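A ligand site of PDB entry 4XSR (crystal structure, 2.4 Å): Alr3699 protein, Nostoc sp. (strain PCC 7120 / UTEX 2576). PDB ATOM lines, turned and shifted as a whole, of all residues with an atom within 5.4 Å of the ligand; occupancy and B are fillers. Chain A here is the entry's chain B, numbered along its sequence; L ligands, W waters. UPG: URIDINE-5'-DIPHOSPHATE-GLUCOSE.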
ATOM      1  N   PRO A  18     -18.735 -16.991 -23.899  1.00  0.00           N
ATOM      2  CA  PRO A  18     -17.582 -17.606 -24.558  1.00  0.00           C
ATOM      3  C   PRO A  18     -16.247 -17.538 -23.761  1.00  0.00           C
ATOM      4  O   PRO A  18     -15.295 -16.840 -24.135  1.00  0.00           O
ATOM      5  CB  PRO A  18     -17.473 -16.804 -25.847  1.00  0.00           C
ATOM      6  CG  PRO A  18     -17.854 -15.427 -25.413  1.00  0.00           C
ATOM      7  CD  PRO A  18     -19.017 -15.670 -24.487  1.00  0.00           C
ATOM      8  N   GLY A  19     -16.197 -18.263 -22.657  1.00  0.00           N
ATOM      9  CA  GLY A  19     -14.976 -18.480 -21.922  1.00  0.00           C
ATOM     10  C   GLY A  19     -14.120 -19.472 -22.692  1.00  0.00           C
ATOM     11  O   GLY A  19     -14.531 -19.974 -23.766  1.00  0.00           O
ATOM     12  N   GLY A  20     -12.940 -19.785 -22.145  1.00  0.00           N
ATOM     13  CA  GLY A  20     -12.020 -20.698 -22.846  1.00  0.00           C
ATOM     14  C   GLY A  20     -12.571 -22.077 -23.140  1.00  0.00           C
ATOM     15  O   GLY A  20     -12.372 -22.643 -24.216  1.00  0.00           O
ATOM     16  N   ALA A  21     -13.269 -22.647 -22.172  1.00  0.00           N
ATOM     17  CA  ALA A  21     -13.817 -23.999 -22.323  1.00  0.00           C
ATOM     18  C   ALA A  21     -14.835 -24.050 -23.446  1.00  0.00           C
ATOM     19  O   ALA A  21     -14.899 -25.005 -24.215  1.00  0.00           O
ATOM     20  CB  ALA A  21     -14.450 -24.417 -21.016  1.00  0.00           C
ATOM     21  N   LEU A  23     -15.023 -21.783 -26.062  1.00  0.00           N
ATOM     22  CA  LEU A  23     -14.360 -21.619 -27.378  1.00  0.00           C
ATOM     23  C   LEU A  23     -13.708 -22.921 -27.749  1.00  0.00           C
ATOM     24  O   LEU A  23     -13.777 -23.342 -28.900  1.00  0.00           O
ATOM     25  CB  LEU A  23     -13.331 -20.493 -27.358  1.00  0.00           C
ATOM     26  CG  LEU A  23     -13.967 -19.151 -26.997  1.00  0.00           C
ATOM     27  CD1 LEU A  23     -12.896 -18.148 -26.649  1.00  0.00           C
ATOM     28  CD2 LEU A  23     -14.841 -18.644 -28.127  1.00  0.00           C
ATOM     29  N   CYS A  24     -13.104 -23.596 -26.765  1.00  0.00           N
ATOM     30  CA  CYS A  24     -12.541 -24.906 -27.059  1.00  0.00           C
ATOM     31  C   CYS A  24     -13.623 -25.854 -27.578  1.00  0.00           C
ATOM     32  O   CYS A  24     -13.385 -26.620 -28.529  1.00  0.00           O
ATOM     33  CB  CYS A  24     -11.866 -25.475 -25.839  1.00  0.00           C
ATOM     34  SG  CYS A  24     -10.956 -26.979 -26.202  1.00  0.00           S
ATOM     35  N   HIS A 127     -11.440 -28.917 -18.117  1.00  0.00           N
ATOM     36  CA  HIS A 127     -10.705 -27.700 -18.462  1.00  0.00           C
ATOM     37  C   HIS A 127     -10.212 -26.948 -17.237  1.00  0.00           C
ATOM     38  O   HIS A 127      -9.639 -25.880 -17.365  1.00  0.00           O
ATOM     39  CB  HIS A 127     -11.596 -26.729 -19.227  1.00  0.00           C
ATOM     40  CG  HIS A 127     -12.094 -27.258 -20.534  1.00  0.00           C
ATOM     41  ND1 HIS A 127     -11.389 -27.119 -21.714  1.00  0.00           N
ATOM     42  CD2 HIS A 127     -13.240 -27.892 -20.859  1.00  0.00           C
ATOM     43  CE1 HIS A 127     -12.068 -27.668 -22.707  1.00  0.00           C
ATOM     44  NE2 HIS A 127     -13.209 -28.137 -22.217  1.00  0.00           N
ATOM     45  N   ASP A 128     -10.422 -27.528 -16.055  1.00  0.00           N
ATOM     46  CA  ASP A 128     -10.057 -26.883 -14.803  1.00  0.00           C
ATOM     47  C   ASP A 128      -8.980 -27.675 -14.116  1.00  0.00           C
ATOM     48  O   ASP A 128      -8.753 -28.836 -14.408  1.00  0.00           O
ATOM     49  CB  ASP A 128     -11.262 -26.792 -13.829  1.00  0.00           C
ATOM     50  CG  ASP A 128     -12.459 -26.020 -14.395  1.00  0.00           C
ATOM     51  OD1 ASP A 128     -12.276 -24.939 -14.999  1.00  0.00           O
ATOM     52  OD2 ASP A 128     -13.607 -26.499 -14.213  1.00  0.00           O
ATOM     53  N   ASN A 157      -7.236 -31.173 -20.289  1.00  0.00           N
ATOM     54  CA  ASN A 157      -6.667 -30.255 -21.283  1.00  0.00           C
ATOM     55  C   ASN A 157      -5.166 -30.061 -21.071  1.00  0.00           C
ATOM     56  O   ASN A 157      -4.533 -29.382 -21.838  1.00  0.00           O
ATOM     57  CB  ASN A 157      -7.379 -28.917 -21.244  1.00  0.00           C
ATOM     58  CG  ASN A 157      -7.252 -28.236 -19.919  1.00  0.00           C
ATOM     59  OD1 ASN A 157      -6.731 -28.809 -18.938  1.00  0.00           O
ATOM     60  ND2 ASN A 157      -7.716 -26.978 -19.869  1.00  0.00           N
ATOM     61  N   ASN A 180      -5.932 -28.253 -26.227  1.00  0.00           N
ATOM     62  CA  ASN A 180      -6.806 -27.517 -27.122  1.00  0.00           C
ATOM     63  C   ASN A 180      -6.208 -27.463 -28.513  1.00  0.00           C
ATOM     64  O   ASN A 180      -4.988 -27.399 -28.673  1.00  0.00           O
ATOM     65  CB  ASN A 180      -6.958 -26.101 -26.690  1.00  0.00           C
ATOM     66  CG  ASN A 180      -7.754 -25.943 -25.436  1.00  0.00           C
ATOM     67  OD1 ASN A 180      -7.843 -26.822 -24.564  1.00  0.00           O
ATOM     68  ND2 ASN A 180      -8.298 -24.770 -25.290  1.00  0.00           N
ATOM     69  N   PHE A 212      -4.736 -10.914 -22.748  1.00  0.00           N
ATOM     70  CA  PHE A 212      -5.951 -11.399 -23.408  1.00  0.00           C
ATOM     71  C   PHE A 212      -6.822 -12.343 -22.551  1.00  0.00           C
ATOM     72  O   PHE A 212      -7.647 -13.088 -23.083  1.00  0.00           O
ATOM     73  CB  PHE A 212      -5.579 -12.068 -24.713  1.00  0.00           C
ATOM     74  CG  PHE A 212      -5.006 -11.105 -25.706  1.00  0.00           C
ATOM     75  CD1 PHE A 212      -3.657 -10.809 -25.700  1.00  0.00           C
ATOM     76  CD2 PHE A 212      -5.821 -10.477 -26.631  1.00  0.00           C
ATOM     77  CE1 PHE A 212      -3.128  -9.920 -26.616  1.00  0.00           C
ATOM     78  CE2 PHE A 212      -5.304  -9.566 -27.526  1.00  0.00           C
ATOM     79  CZ  PHE A 212      -3.955  -9.296 -27.534  1.00  0.00           C
ATOM     80  N   SER A 213      -6.651 -12.239 -21.238  1.00  0.00           N
ATOM     81  CA  SER A 213      -7.433 -13.004 -20.289  1.00  0.00           C
ATOM     82  C   SER A 213      -8.685 -12.206 -19.861  1.00  0.00           C
ATOM     83  O   SER A 213      -8.633 -10.975 -19.692  1.00  0.00           O
ATOM     84  CB  SER A 213      -6.583 -13.297 -19.053  1.00  0.00           C
ATOM     85  OG  SER A 213      -5.402 -14.006 -19.396  1.00  0.00           O
ATOM     86  N   ARG A 214      -9.798 -12.922 -19.654  1.00  0.00           N
ATOM     87  CA  ARG A 214     -10.953 -12.320 -18.991  1.00  0.00           C
ATOM     88  C   ARG A 214     -10.491 -11.639 -17.696  1.00  0.00           C
ATOM     89  O   ARG A 214      -9.512 -12.044 -17.110  1.00  0.00           O
ATOM     90  CB  ARG A 214     -12.059 -13.375 -18.716  1.00  0.00           C
ATOM     91  CG  ARG A 214     -12.034 -14.047 -17.325  1.00  0.00           C
ATOM     92  CD  ARG A 214     -12.883 -15.333 -17.289  1.00  0.00           C
ATOM     93  NE  ARG A 214     -12.654 -16.218 -16.129  1.00  0.00           N
ATOM     94  CZ  ARG A 214     -12.399 -17.535 -16.183  1.00  0.00           C
ATOM     95  NH1 ARG A 214     -12.230 -18.240 -15.049  1.00  0.00           N
ATOM     96  NH2 ARG A 214     -12.312 -18.193 -17.347  1.00  0.00           N
ATOM     97  N   TRP A 218      -7.593 -13.753 -10.483  1.00  0.00           N
ATOM     98  CA  TRP A 218      -6.635 -14.825 -10.655  1.00  0.00           C
ATOM     99  C   TRP A 218      -5.969 -14.786 -12.035  1.00  0.00           C
ATOM    100  O   TRP A 218      -4.904 -15.395 -12.228  1.00  0.00           O
ATOM    101  CB  TRP A 218      -7.249 -16.204 -10.363  1.00  0.00           C
ATOM    102  CG  TRP A 218      -7.994 -16.853 -11.472  1.00  0.00           C
ATOM    103  CD1 TRP A 218      -9.341 -16.739 -11.750  1.00  0.00           C
ATOM    104  CD2 TRP A 218      -7.455 -17.746 -12.446  1.00  0.00           C
ATOM    105  NE1 TRP A 218      -9.664 -17.499 -12.865  1.00  0.00           N
ATOM    106  CE2 TRP A 218      -8.530 -18.139 -13.299  1.00  0.00           C
ATOM    107  CE3 TRP A 218      -6.180 -18.272 -12.680  1.00  0.00           C
ATOM    108  CZ2 TRP A 218      -8.346 -19.028 -14.339  1.00  0.00           C
ATOM    109  CZ3 TRP A 218      -6.001 -19.134 -13.731  1.00  0.00           C
ATOM    110  CH2 TRP A 218      -7.078 -19.505 -14.561  1.00  0.00           C
ATOM    111  N   LYS A 219      -6.566 -14.072 -12.986  1.00  0.00           N
ATOM    112  CA  LYS A 219      -5.883 -13.866 -14.275  1.00  0.00           C
ATOM    113  C   LYS A 219      -4.776 -12.765 -14.202  1.00  0.00           C
ATOM    114  O   LYS A 219      -4.015 -12.586 -15.150  1.00  0.00           O
ATOM    115  CB  LYS A 219      -6.862 -13.561 -15.388  1.00  0.00           C
ATOM    116  CG  LYS A 219      -7.799 -14.691 -15.744  1.00  0.00           C
ATOM    117  CD  LYS A 219      -7.087 -15.914 -16.267  1.00  0.00           C
ATOM    118  CE  LYS A 219      -8.071 -16.853 -16.953  1.00  0.00           C
ATOM    119  NZ  LYS A 219      -7.448 -17.868 -17.841  1.00  0.00           N
ATOM    120  N   VAL A 240      -7.339  -6.889 -23.024  1.00  0.00           N
ATOM    121  CA  VAL A 240      -8.443  -7.367 -23.825  1.00  0.00           C
ATOM    122  C   VAL A 240      -9.247  -8.457 -23.097  1.00  0.00           C
ATOM    123  O   VAL A 240      -8.695  -9.495 -22.697  1.00  0.00           O
ATOM    124  CB  VAL A 240      -7.928  -7.894 -25.158  1.00  0.00           C
ATOM    125  CG1 VAL A 240      -9.074  -8.190 -26.118  1.00  0.00           C
ATOM    126  CG2 VAL A 240      -6.968  -6.887 -25.785  1.00  0.00           C
ATOM    127  N   GLY A 241     -10.550  -8.231 -22.957  1.00  0.00           N
ATOM    128  CA  GLY A 241     -11.467  -9.131 -22.252  1.00  0.00           C
ATOM    129  C   GLY A 241     -12.370  -8.328 -21.338  1.00  0.00           C
ATOM    130  O   GLY A 241     -12.046  -7.181 -21.039  1.00  0.00           O
ATOM    131  N   ASP A 242     -13.504  -8.894 -20.920  1.00  0.00           N
ATOM    132  CA  ASP A 242     -14.395  -8.192 -19.963  1.00  0.00           C
ATOM    133  C   ASP A 242     -14.460  -8.988 -18.682  1.00  0.00           C
ATOM    134  O   ASP A 242     -13.931 -10.093 -18.635  1.00  0.00           O
ATOM    135  CB  ASP A 242     -15.812  -7.931 -20.528  1.00  0.00           C
ATOM    136  CG  ASP A 242     -16.534  -9.216 -20.991  1.00  0.00           C
ATOM    137  OD1 ASP A 242     -15.983 -10.345 -20.917  1.00  0.00           O
ATOM    138  OD2 ASP A 242     -17.695  -9.077 -21.462  1.00  0.00           O
ATOM    139  N   LEU A 244     -16.120 -11.421 -17.001  1.00  0.00           N
ATOM    140  CA  LEU A 244     -17.106 -12.399 -17.546  1.00  0.00           C
ATOM    141  C   LEU A 244     -18.148 -12.840 -16.495  1.00  0.00           C
ATOM    142  O   LEU A 244     -19.218 -13.339 -16.881  1.00  0.00           O
ATOM    143  CB  LEU A 244     -16.420 -13.676 -18.161  1.00  0.00           C
ATOM    144  CG  LEU A 244     -15.801 -13.704 -19.589  1.00  0.00           C
ATOM    145  CD1 LEU A 244     -15.095 -15.020 -19.930  1.00  0.00           C
ATOM    146  CD2 LEU A 244     -16.842 -13.413 -20.655  1.00  0.00           C
ATOM    147  N   GLY A 271     -12.414  -4.146 -23.844  1.00  0.00           N
ATOM    148  CA  GLY A 271     -13.538  -5.053 -23.659  1.00  0.00           C
ATOM    149  C   GLY A 271     -13.355  -6.380 -24.395  1.00  0.00           C
ATOM    150  O   GLY A 271     -12.290  -6.662 -24.938  1.00  0.00           O
ATOM    151  N   PHE A 272     -14.399  -7.204 -24.412  1.00  0.00           N
ATOM    152  CA  PHE A 272     -14.328  -8.459 -25.117  1.00  0.00           C
ATOM    153  C   PHE A 272     -14.252  -8.163 -26.562  1.00  0.00           C
ATOM    154  O   PHE A 272     -15.040  -7.416 -27.083  1.00  0.00           O
ATOM    155  CB  PHE A 272     -15.540  -9.352 -24.854  1.00  0.00           C
ATOM    156  CG  PHE A 272     -15.290 -10.805 -25.234  1.00  0.00           C
ATOM    157  CD1 PHE A 272     -14.674 -11.689 -24.344  1.00  0.00           C
ATOM    158  CD2 PHE A 272     -15.657 -11.284 -26.504  1.00  0.00           C
ATOM    159  CE1 PHE A 272     -14.441 -13.016 -24.686  1.00  0.00           C
ATOM    160  CE2 PHE A 272     -15.431 -12.614 -26.861  1.00  0.00           C
ATOM    161  CZ  PHE A 272     -14.816 -13.480 -25.962  1.00  0.00           C
ATOM    162  N   ARG A 273     -13.304  -8.800 -27.228  1.00  0.00           N
ATOM    163  CA  ARG A 273     -13.069  -8.616 -28.645  1.00  0.00           C
ATOM    164  C   ARG A 273     -13.050  -9.956 -29.384  1.00  0.00           C
ATOM    165  O   ARG A 273     -12.688 -10.987 -28.810  1.00  0.00           O
ATOM    166  CB  ARG A 273     -11.715  -7.926 -28.791  1.00  0.00           C
ATOM    167  CG  ARG A 273     -11.776  -6.419 -28.554  1.00  0.00           C
ATOM    168  CD  ARG A 273     -12.210  -5.746 -29.854  1.00  0.00           C
ATOM    169  NE  ARG A 273     -11.764  -4.369 -29.889  1.00  0.00           N
ATOM    170  CZ  ARG A 273     -10.966  -3.812 -30.804  1.00  0.00           C
ATOM    171  NH1 ARG A 273     -10.480  -4.470 -31.865  1.00  0.00           N
ATOM    172  NH2 ARG A 273     -10.661  -2.535 -30.649  1.00  0.00           N
ATOM    173  N   ALA A 274     -13.400  -9.911 -30.666  1.00  0.00           N
ATOM    174  CA  ALA A 274     -13.377 -11.077 -31.545  1.00  0.00           C
ATOM    175  C   ALA A 274     -12.165 -11.157 -32.454  1.00  0.00           C
ATOM    176  O   ALA A 274     -11.878 -12.204 -33.029  1.00  0.00           O
ATOM    177  CB  ALA A 274     -14.639 -11.065 -32.409  1.00  0.00           C
ATOM    178  N   ILE A 276      -8.903 -11.385 -32.157  1.00  0.00           N
ATOM    179  CA  ILE A 276      -7.759 -11.667 -31.280  1.00  0.00           C
ATOM    180  C   ILE A 276      -6.445 -11.884 -32.048  1.00  0.00           C
ATOM    181  O   ILE A 276      -5.427 -11.289 -31.718  1.00  0.00           O
ATOM    182  CB  ILE A 276      -8.046 -12.841 -30.323  1.00  0.00           C
ATOM    183  CG1 ILE A 276      -9.264 -12.528 -29.433  1.00  0.00           C
ATOM    184  CG2 ILE A 276      -6.847 -13.106 -29.411  1.00  0.00           C
ATOM    185  CD1 ILE A 276      -9.160 -11.234 -28.663  1.00  0.00           C
ATOM    186  N   MET A 280      -3.324  -9.482 -31.447  1.00  0.00           N
ATOM    187  CA  MET A 280      -2.044 -10.056 -30.999  1.00  0.00           C
ATOM    188  C   MET A 280      -0.915  -9.639 -31.936  1.00  0.00           C
ATOM    189  O   MET A 280       0.157  -9.299 -31.482  1.00  0.00           O
ATOM    190  CB  MET A 280      -2.100 -11.572 -30.878  1.00  0.00           C
ATOM    191  CG  MET A 280      -2.820 -12.026 -29.612  1.00  0.00           C
ATOM    192  SD  MET A 280      -2.724 -13.815 -29.455  1.00  0.00           S
ATOM    193  CE  MET A 280      -3.664 -13.983 -27.946  1.00  0.00           C
ATOM    194  N   GLU A 294      -2.583 -21.922 -14.312  1.00  0.00           N
ATOM    195  CA  GLU A 294      -3.399 -21.985 -15.469  1.00  0.00           C
ATOM    196  C   GLU A 294      -3.507 -23.401 -15.934  1.00  0.00           C
ATOM    197  O   GLU A 294      -2.525 -24.080 -16.104  1.00  0.00           O
ATOM    198  CB  GLU A 294      -2.835 -21.109 -16.556  1.00  0.00           C
ATOM    199  CG  GLU A 294      -3.723 -20.926 -17.755  1.00  0.00           C
ATOM    200  CD  GLU A 294      -4.852 -19.967 -17.501  1.00  0.00           C
ATOM    201  OE1 GLU A 294      -4.636 -18.958 -16.896  1.00  0.00           O
ATOM    202  OE2 GLU A 294      -5.956 -20.225 -17.920  1.00  0.00           O
ATOM    203  N   PRO A 295      -4.710 -23.853 -16.157  1.00  0.00           N
ATOM    204  CA  PRO A 295      -4.905 -25.213 -16.626  1.00  0.00           C
ATOM    205  C   PRO A 295      -4.330 -25.449 -17.978  1.00  0.00           C
ATOM    206  O   PRO A 295      -3.669 -26.402 -18.153  1.00  0.00           O
ATOM    207  CB  PRO A 295      -6.409 -25.315 -16.687  1.00  0.00           C
ATOM    208  CG  PRO A 295      -6.869 -24.458 -15.619  1.00  0.00           C
ATOM    209  CD  PRO A 295      -5.925 -23.303 -15.571  1.00  0.00           C
ATOM    210  N   PHE A 296      -4.565 -24.573 -18.924  1.00  0.00           N
ATOM    211  CA  PHE A 296      -3.956 -24.737 -20.217  1.00  0.00           C
ATOM    212  C   PHE A 296      -3.297 -23.456 -20.709  1.00  0.00           C
ATOM    213  O   PHE A 296      -2.101 -23.366 -20.747  1.00  0.00           O
ATOM    214  CB  PHE A 296      -4.948 -25.255 -21.218  1.00  0.00           C
ATOM    215  CG  PHE A 296      -4.387 -25.440 -22.581  1.00  0.00           C
ATOM    216  CD1 PHE A 296      -3.622 -26.516 -22.862  1.00  0.00           C
ATOM    217  CD2 PHE A 296      -4.640 -24.539 -23.576  1.00  0.00           C
ATOM    218  CE1 PHE A 296      -3.116 -26.704 -24.114  1.00  0.00           C
ATOM    219  CE2 PHE A 296      -4.144 -24.717 -24.825  1.00  0.00           C
ATOM    220  CZ  PHE A 296      -3.371 -25.807 -25.101  1.00  0.00           C
ATOM    221  N   GLY A 297      -4.099 -22.462 -21.012  1.00  0.00           N
ATOM    222  CA  GLY A 297      -3.664 -21.180 -21.516  1.00  0.00           C
ATOM    223  C   GLY A 297      -3.750 -20.986 -23.010  1.00  0.00           C
ATOM    224  O   GLY A 297      -2.809 -21.132 -23.734  1.00  0.00           O
ATOM    225  N   ARG A 298      -4.941 -20.670 -23.454  1.00  0.00           N
ATOM    226  CA  ARG A 298      -5.181 -20.492 -24.858  1.00  0.00           C
ATOM    227  C   ARG A 298      -4.428 -19.316 -25.404  1.00  0.00           C
ATOM    228  O   ARG A 298      -3.917 -19.361 -26.475  1.00  0.00           O
ATOM    229  CB  ARG A 298      -6.662 -20.345 -25.118  1.00  0.00           C
ATOM    230  CG  ARG A 298      -7.369 -21.655 -25.138  1.00  0.00           C
ATOM    231  CD  ARG A 298      -8.861 -21.471 -25.186  1.00  0.00           C
ATOM    232  NE  ARG A 298      -9.287 -21.122 -26.514  1.00  0.00           N
ATOM    233  CZ  ARG A 298      -9.421 -21.981 -27.493  1.00  0.00           C
ATOM    234  NH1 ARG A 298      -9.192 -23.244 -27.305  1.00  0.00           N
ATOM    235  NH2 ARG A 298      -9.803 -21.568 -28.661  1.00  0.00           N
ATOM    236  N   VAL A 299      -4.386 -18.251 -24.630  1.00  0.00           N
ATOM    237  CA  VAL A 299      -3.815 -17.047 -25.174  1.00  0.00           C
ATOM    238  C   VAL A 299      -2.334 -17.302 -25.491  1.00  0.00           C
ATOM    239  O   VAL A 299      -1.816 -16.717 -26.429  1.00  0.00           O
ATOM    240  CB  VAL A 299      -4.010 -15.822 -24.285  1.00  0.00           C
ATOM    241  CG1 VAL A 299      -5.469 -15.720 -23.846  1.00  0.00           C
ATOM    242  CG2 VAL A 299      -3.064 -15.852 -23.096  1.00  0.00           C
ATOM    243  N   GLU A 302      -2.076 -19.075 -28.743  1.00  0.00           N
ATOM    244  CA  GLU A 302      -2.557 -18.163 -29.768  1.00  0.00           C
ATOM    245  C   GLU A 302      -1.424 -17.175 -30.152  1.00  0.00           C
ATOM    246  O   GLU A 302      -1.173 -16.944 -31.332  1.00  0.00           O
ATOM    247  CB  GLU A 302      -3.838 -17.457 -29.292  1.00  0.00           C
ATOM    248  CG  GLU A 302      -5.096 -18.365 -29.350  1.00  0.00           C
ATOM    249  CD  GLU A 302      -6.308 -17.857 -28.554  1.00  0.00           C
ATOM    250  OE1 GLU A 302      -7.405 -18.437 -28.654  1.00  0.00           O
ATOM    251  OE2 GLU A 302      -6.192 -16.860 -27.819  1.00  0.00           O
HETATM  252  N1  UPG L   1     -10.584 -14.211 -25.851  1.00  0.00           N
HETATM  253  C2  UPG L   1     -11.424 -13.591 -26.763  1.00  0.00           C
HETATM  254  N3  UPG L   1     -11.757 -12.301 -26.593  1.00  0.00           N
HETATM  255  C4  UPG L   1     -11.332 -11.602 -25.552  1.00  0.00           C
HETATM  256  C5  UPG L   1     -10.531 -12.211 -24.598  1.00  0.00           C
HETATM  257  C6  UPG L   1     -10.158 -13.540 -24.778  1.00  0.00           C
HETATM  258  O2  UPG L   1     -11.835 -14.247 -27.755  1.00  0.00           O
HETATM  259  O4  UPG L   1     -11.670 -10.405 -25.444  1.00  0.00           O
HETATM  260  C1C UPG L   1     -10.258 -15.608 -26.032  1.00  0.00           C
HETATM  261  C2C UPG L   1      -8.780 -15.884 -26.198  1.00  0.00           C
HETATM  262  O2C UPG L   1      -8.369 -15.733 -27.587  1.00  0.00           O
HETATM  263  C3C UPG L   1      -8.733 -17.310 -25.657  1.00  0.00           C
HETATM  264  C4C UPG L   1      -9.819 -17.379 -24.585  1.00  0.00           C
HETATM  265  O4C UPG L   1     -10.675 -16.270 -24.830  1.00  0.00           O
HETATM  266  O3C UPG L   1      -9.134 -18.208 -26.703  1.00  0.00           O
HETATM  267  C5C UPG L   1      -9.334 -17.273 -23.155  1.00  0.00           C
HETATM  268  O5C UPG L   1      -8.813 -18.570 -22.909  1.00  0.00           O
HETATM  269  PA  UPG L   1      -8.251 -18.973 -21.471  1.00  0.00           P
HETATM  270  O1A UPG L   1      -7.249 -20.013 -21.834  1.00  0.00           O
HETATM  271  O2A UPG L   1      -8.008 -17.843 -20.553  1.00  0.00           O
HETATM  272  O3A UPG L   1      -9.527 -19.835 -20.988  1.00  0.00           O
HETATM  273  PB  UPG L   1     -10.333 -19.840 -19.614  1.00  0.00           P
HETATM  274  O1B UPG L   1      -9.587 -19.545 -18.366  1.00  0.00           O
HETATM  275  O2B UPG L   1     -11.530 -18.958 -19.892  1.00  0.00           O
HETATM  276  O3B UPG L   1     -10.805 -21.392 -19.724  1.00  0.00           O
HETATM  277  C1' UPG L   1     -10.395 -22.625 -19.126  1.00  0.00           C
HETATM  278  C2' UPG L   1      -9.068 -22.644 -18.423  1.00  0.00           C
HETATM  279  C3' UPG L   1      -7.938 -22.289 -19.392  1.00  0.00           C
HETATM  280  C4' UPG L   1      -7.998 -23.198 -20.599  1.00  0.00           C
HETATM  281  C5' UPG L   1      -9.412 -23.224 -21.197  1.00  0.00           C
HETATM  282  C6' UPG L   1      -9.481 -24.202 -22.338  1.00  0.00           C
HETATM  283  O2' UPG L   1      -9.091 -21.830 -17.253  1.00  0.00           O
HETATM  284  O3' UPG L   1      -6.695 -22.555 -18.735  1.00  0.00           O
HETATM  285  O4' UPG L   1      -7.064 -22.764 -21.577  1.00  0.00           O
HETATM  286  O5' UPG L   1     -10.327 -23.598 -20.183  1.00  0.00           O
HETATM  287  O6' UPG L   1      -9.074 -25.511 -21.897  1.00  0.00           O
HETATM  288  O   HOH W   1      -5.728 -16.727 -19.763  1.00  0.00           O
HETATM  289  O   HOH W   2     -10.367 -23.071 -15.095  1.00  0.00           O
HETATM  290  O   HOH W   3      -9.570 -15.790 -19.887  1.00  0.00           O
HETATM  291  O   HOH W   4     -12.889 -15.992 -23.083  1.00  0.00           O
HETATM  292  O   HOH W   5     -13.062 -14.884 -30.740  1.00  0.00           O
HETATM  293  O   HOH W   6     -10.339 -18.449 -29.823  1.00  0.00           O
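OE2 of Glu 302 sits at hydrogen-bond distance from O2C of the ligand (2.5 Å).
The side-chain carboxylate of Glu 294 is in hydrogen-bond range of an oxygen (O3') of the ligand.
O4 of the ligand lies within hydrogen-bond range of N of Arg 273 (2.9 Å).
A nitrogen (N3) of the ligand is in hydrogen-bond range of the backbone carbonyl oxygen of Arg 273, at 2.7 Å.
The side-chain amino group (NZ) of Lys 219 is in salt-bridge range of an oxygen (O1B) of the ligand (2.8 Å).
NH2 of Arg 214 is in salt-bridge range of O2B of the ligand, 2.8 Å away.
An oxygen (O2B) of the ligand sits at hydrogen-bond distance from the backbone NH (N) of Gly 20.
An oxygen (O6') of the ligand lies within hydrogen-bond range of a ring nitrogen (ND1) of His 127 (2.8 Å).
An oxygen (O6') of the ligand lies within hydrogen-bond range of the side-chain amide nitrogen (ND2) of Asn 157, 2.8 Å away.
The backbone NH (N) of Arg 298 lies within hydrogen-bond range of an oxygen (O1A) of the ligand, at 2.9 Å.
An oxygen (O3C) of the ligand is in hydrogen-bond range of the guanidinium group of Arg 298, at 2.9 Å.
The backbone NH of Phe 296 lies within hydrogen-bond range of an oxygen (O3') of the ligand (2.9 Å).
The backbone NH (N) of Gly 297 lies within hydrogen-bond range of an oxygen (O4') of the ligand, at 3.0 Å.
An oxygen (O6') of the ligand lies within hydrogen-bond range of the side-chain amide oxygen (OD1) of Asn 180 (3.2 Å).
The backbone NH (N) of Gly 241 sits close to an oxygen (O4) of the ligand (3.5 Å).
Merely in contact with the ligand: Phe 212, Phe 272, Pro 295, Leu 23, Val 240, Ile 276, Ala 21, Gly 271 and Gly 19.
Hydrophobic or aromatic side chains that line the ligand: Leu 23, His 127, Val 240, Phe 272, Ile 276, Pro 295 and Phe 296.
Of the 32 residues printed, 22 come within 4 Å of the ligand.
The nearest printed residue that does not touch the ligand is Val 299 (4.1 Å).
Water W1 lies within hydrogen-bond range of O2A of the ligand (2.7 Å), OG of Ser 213 (2.8 Å) and NZ of Lys 219 (2.8 Å).
Water W3 bridges O2A of the ligand (2.7 Å) and N of Arg 214 (2.9 Å).
Water W2 bridges the side-chain carboxylate (OD1) of Asp 128 (2.7 Å) and an oxygen (O2') of the ligand (2.8 Å).
Water W4 bridges the backbone carbonyl oxygen of Pro 18 (2.8 Å) and an oxygen (O4C) of the ligand (2.8 Å).
Water W6 lies within hydrogen-bond range of the side-chain carboxylate of Glu 302 (3.2 Å), an oxygen (O3C) of the ligand (3.4 Å) and the guanidinium group of Arg 298 (3.4 Å).
OE1 of Glu 302 is in salt-bridge range of NE of Arg 298, 3.9 Å away.
The side-chain carboxylate (OE2) of Glu 294 is in salt-bridge range of the side-chain amino group (NZ) of Lys 219, 2.8 Å away.
The backbone carbonyl oxygen of His 127 is in hydrogen-bond range of the side-chain amide nitrogen of Asn 157 (3.3 Å).
The guanidinium group (NH1) of Arg 298 sits close to the side-chain amide nitrogen (ND2) of Asn 180 (2.7 Å).
The side-chain sulfur (SG) of Cys 24 lies close to the side-chain amide oxygen (OD1) of Asn 180, at 3.5 Å.
The backbone carbonyl oxygen of Gly 271 lies within hydrogen-bond range of the backbone NH of Gly 241 (3.1 Å).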
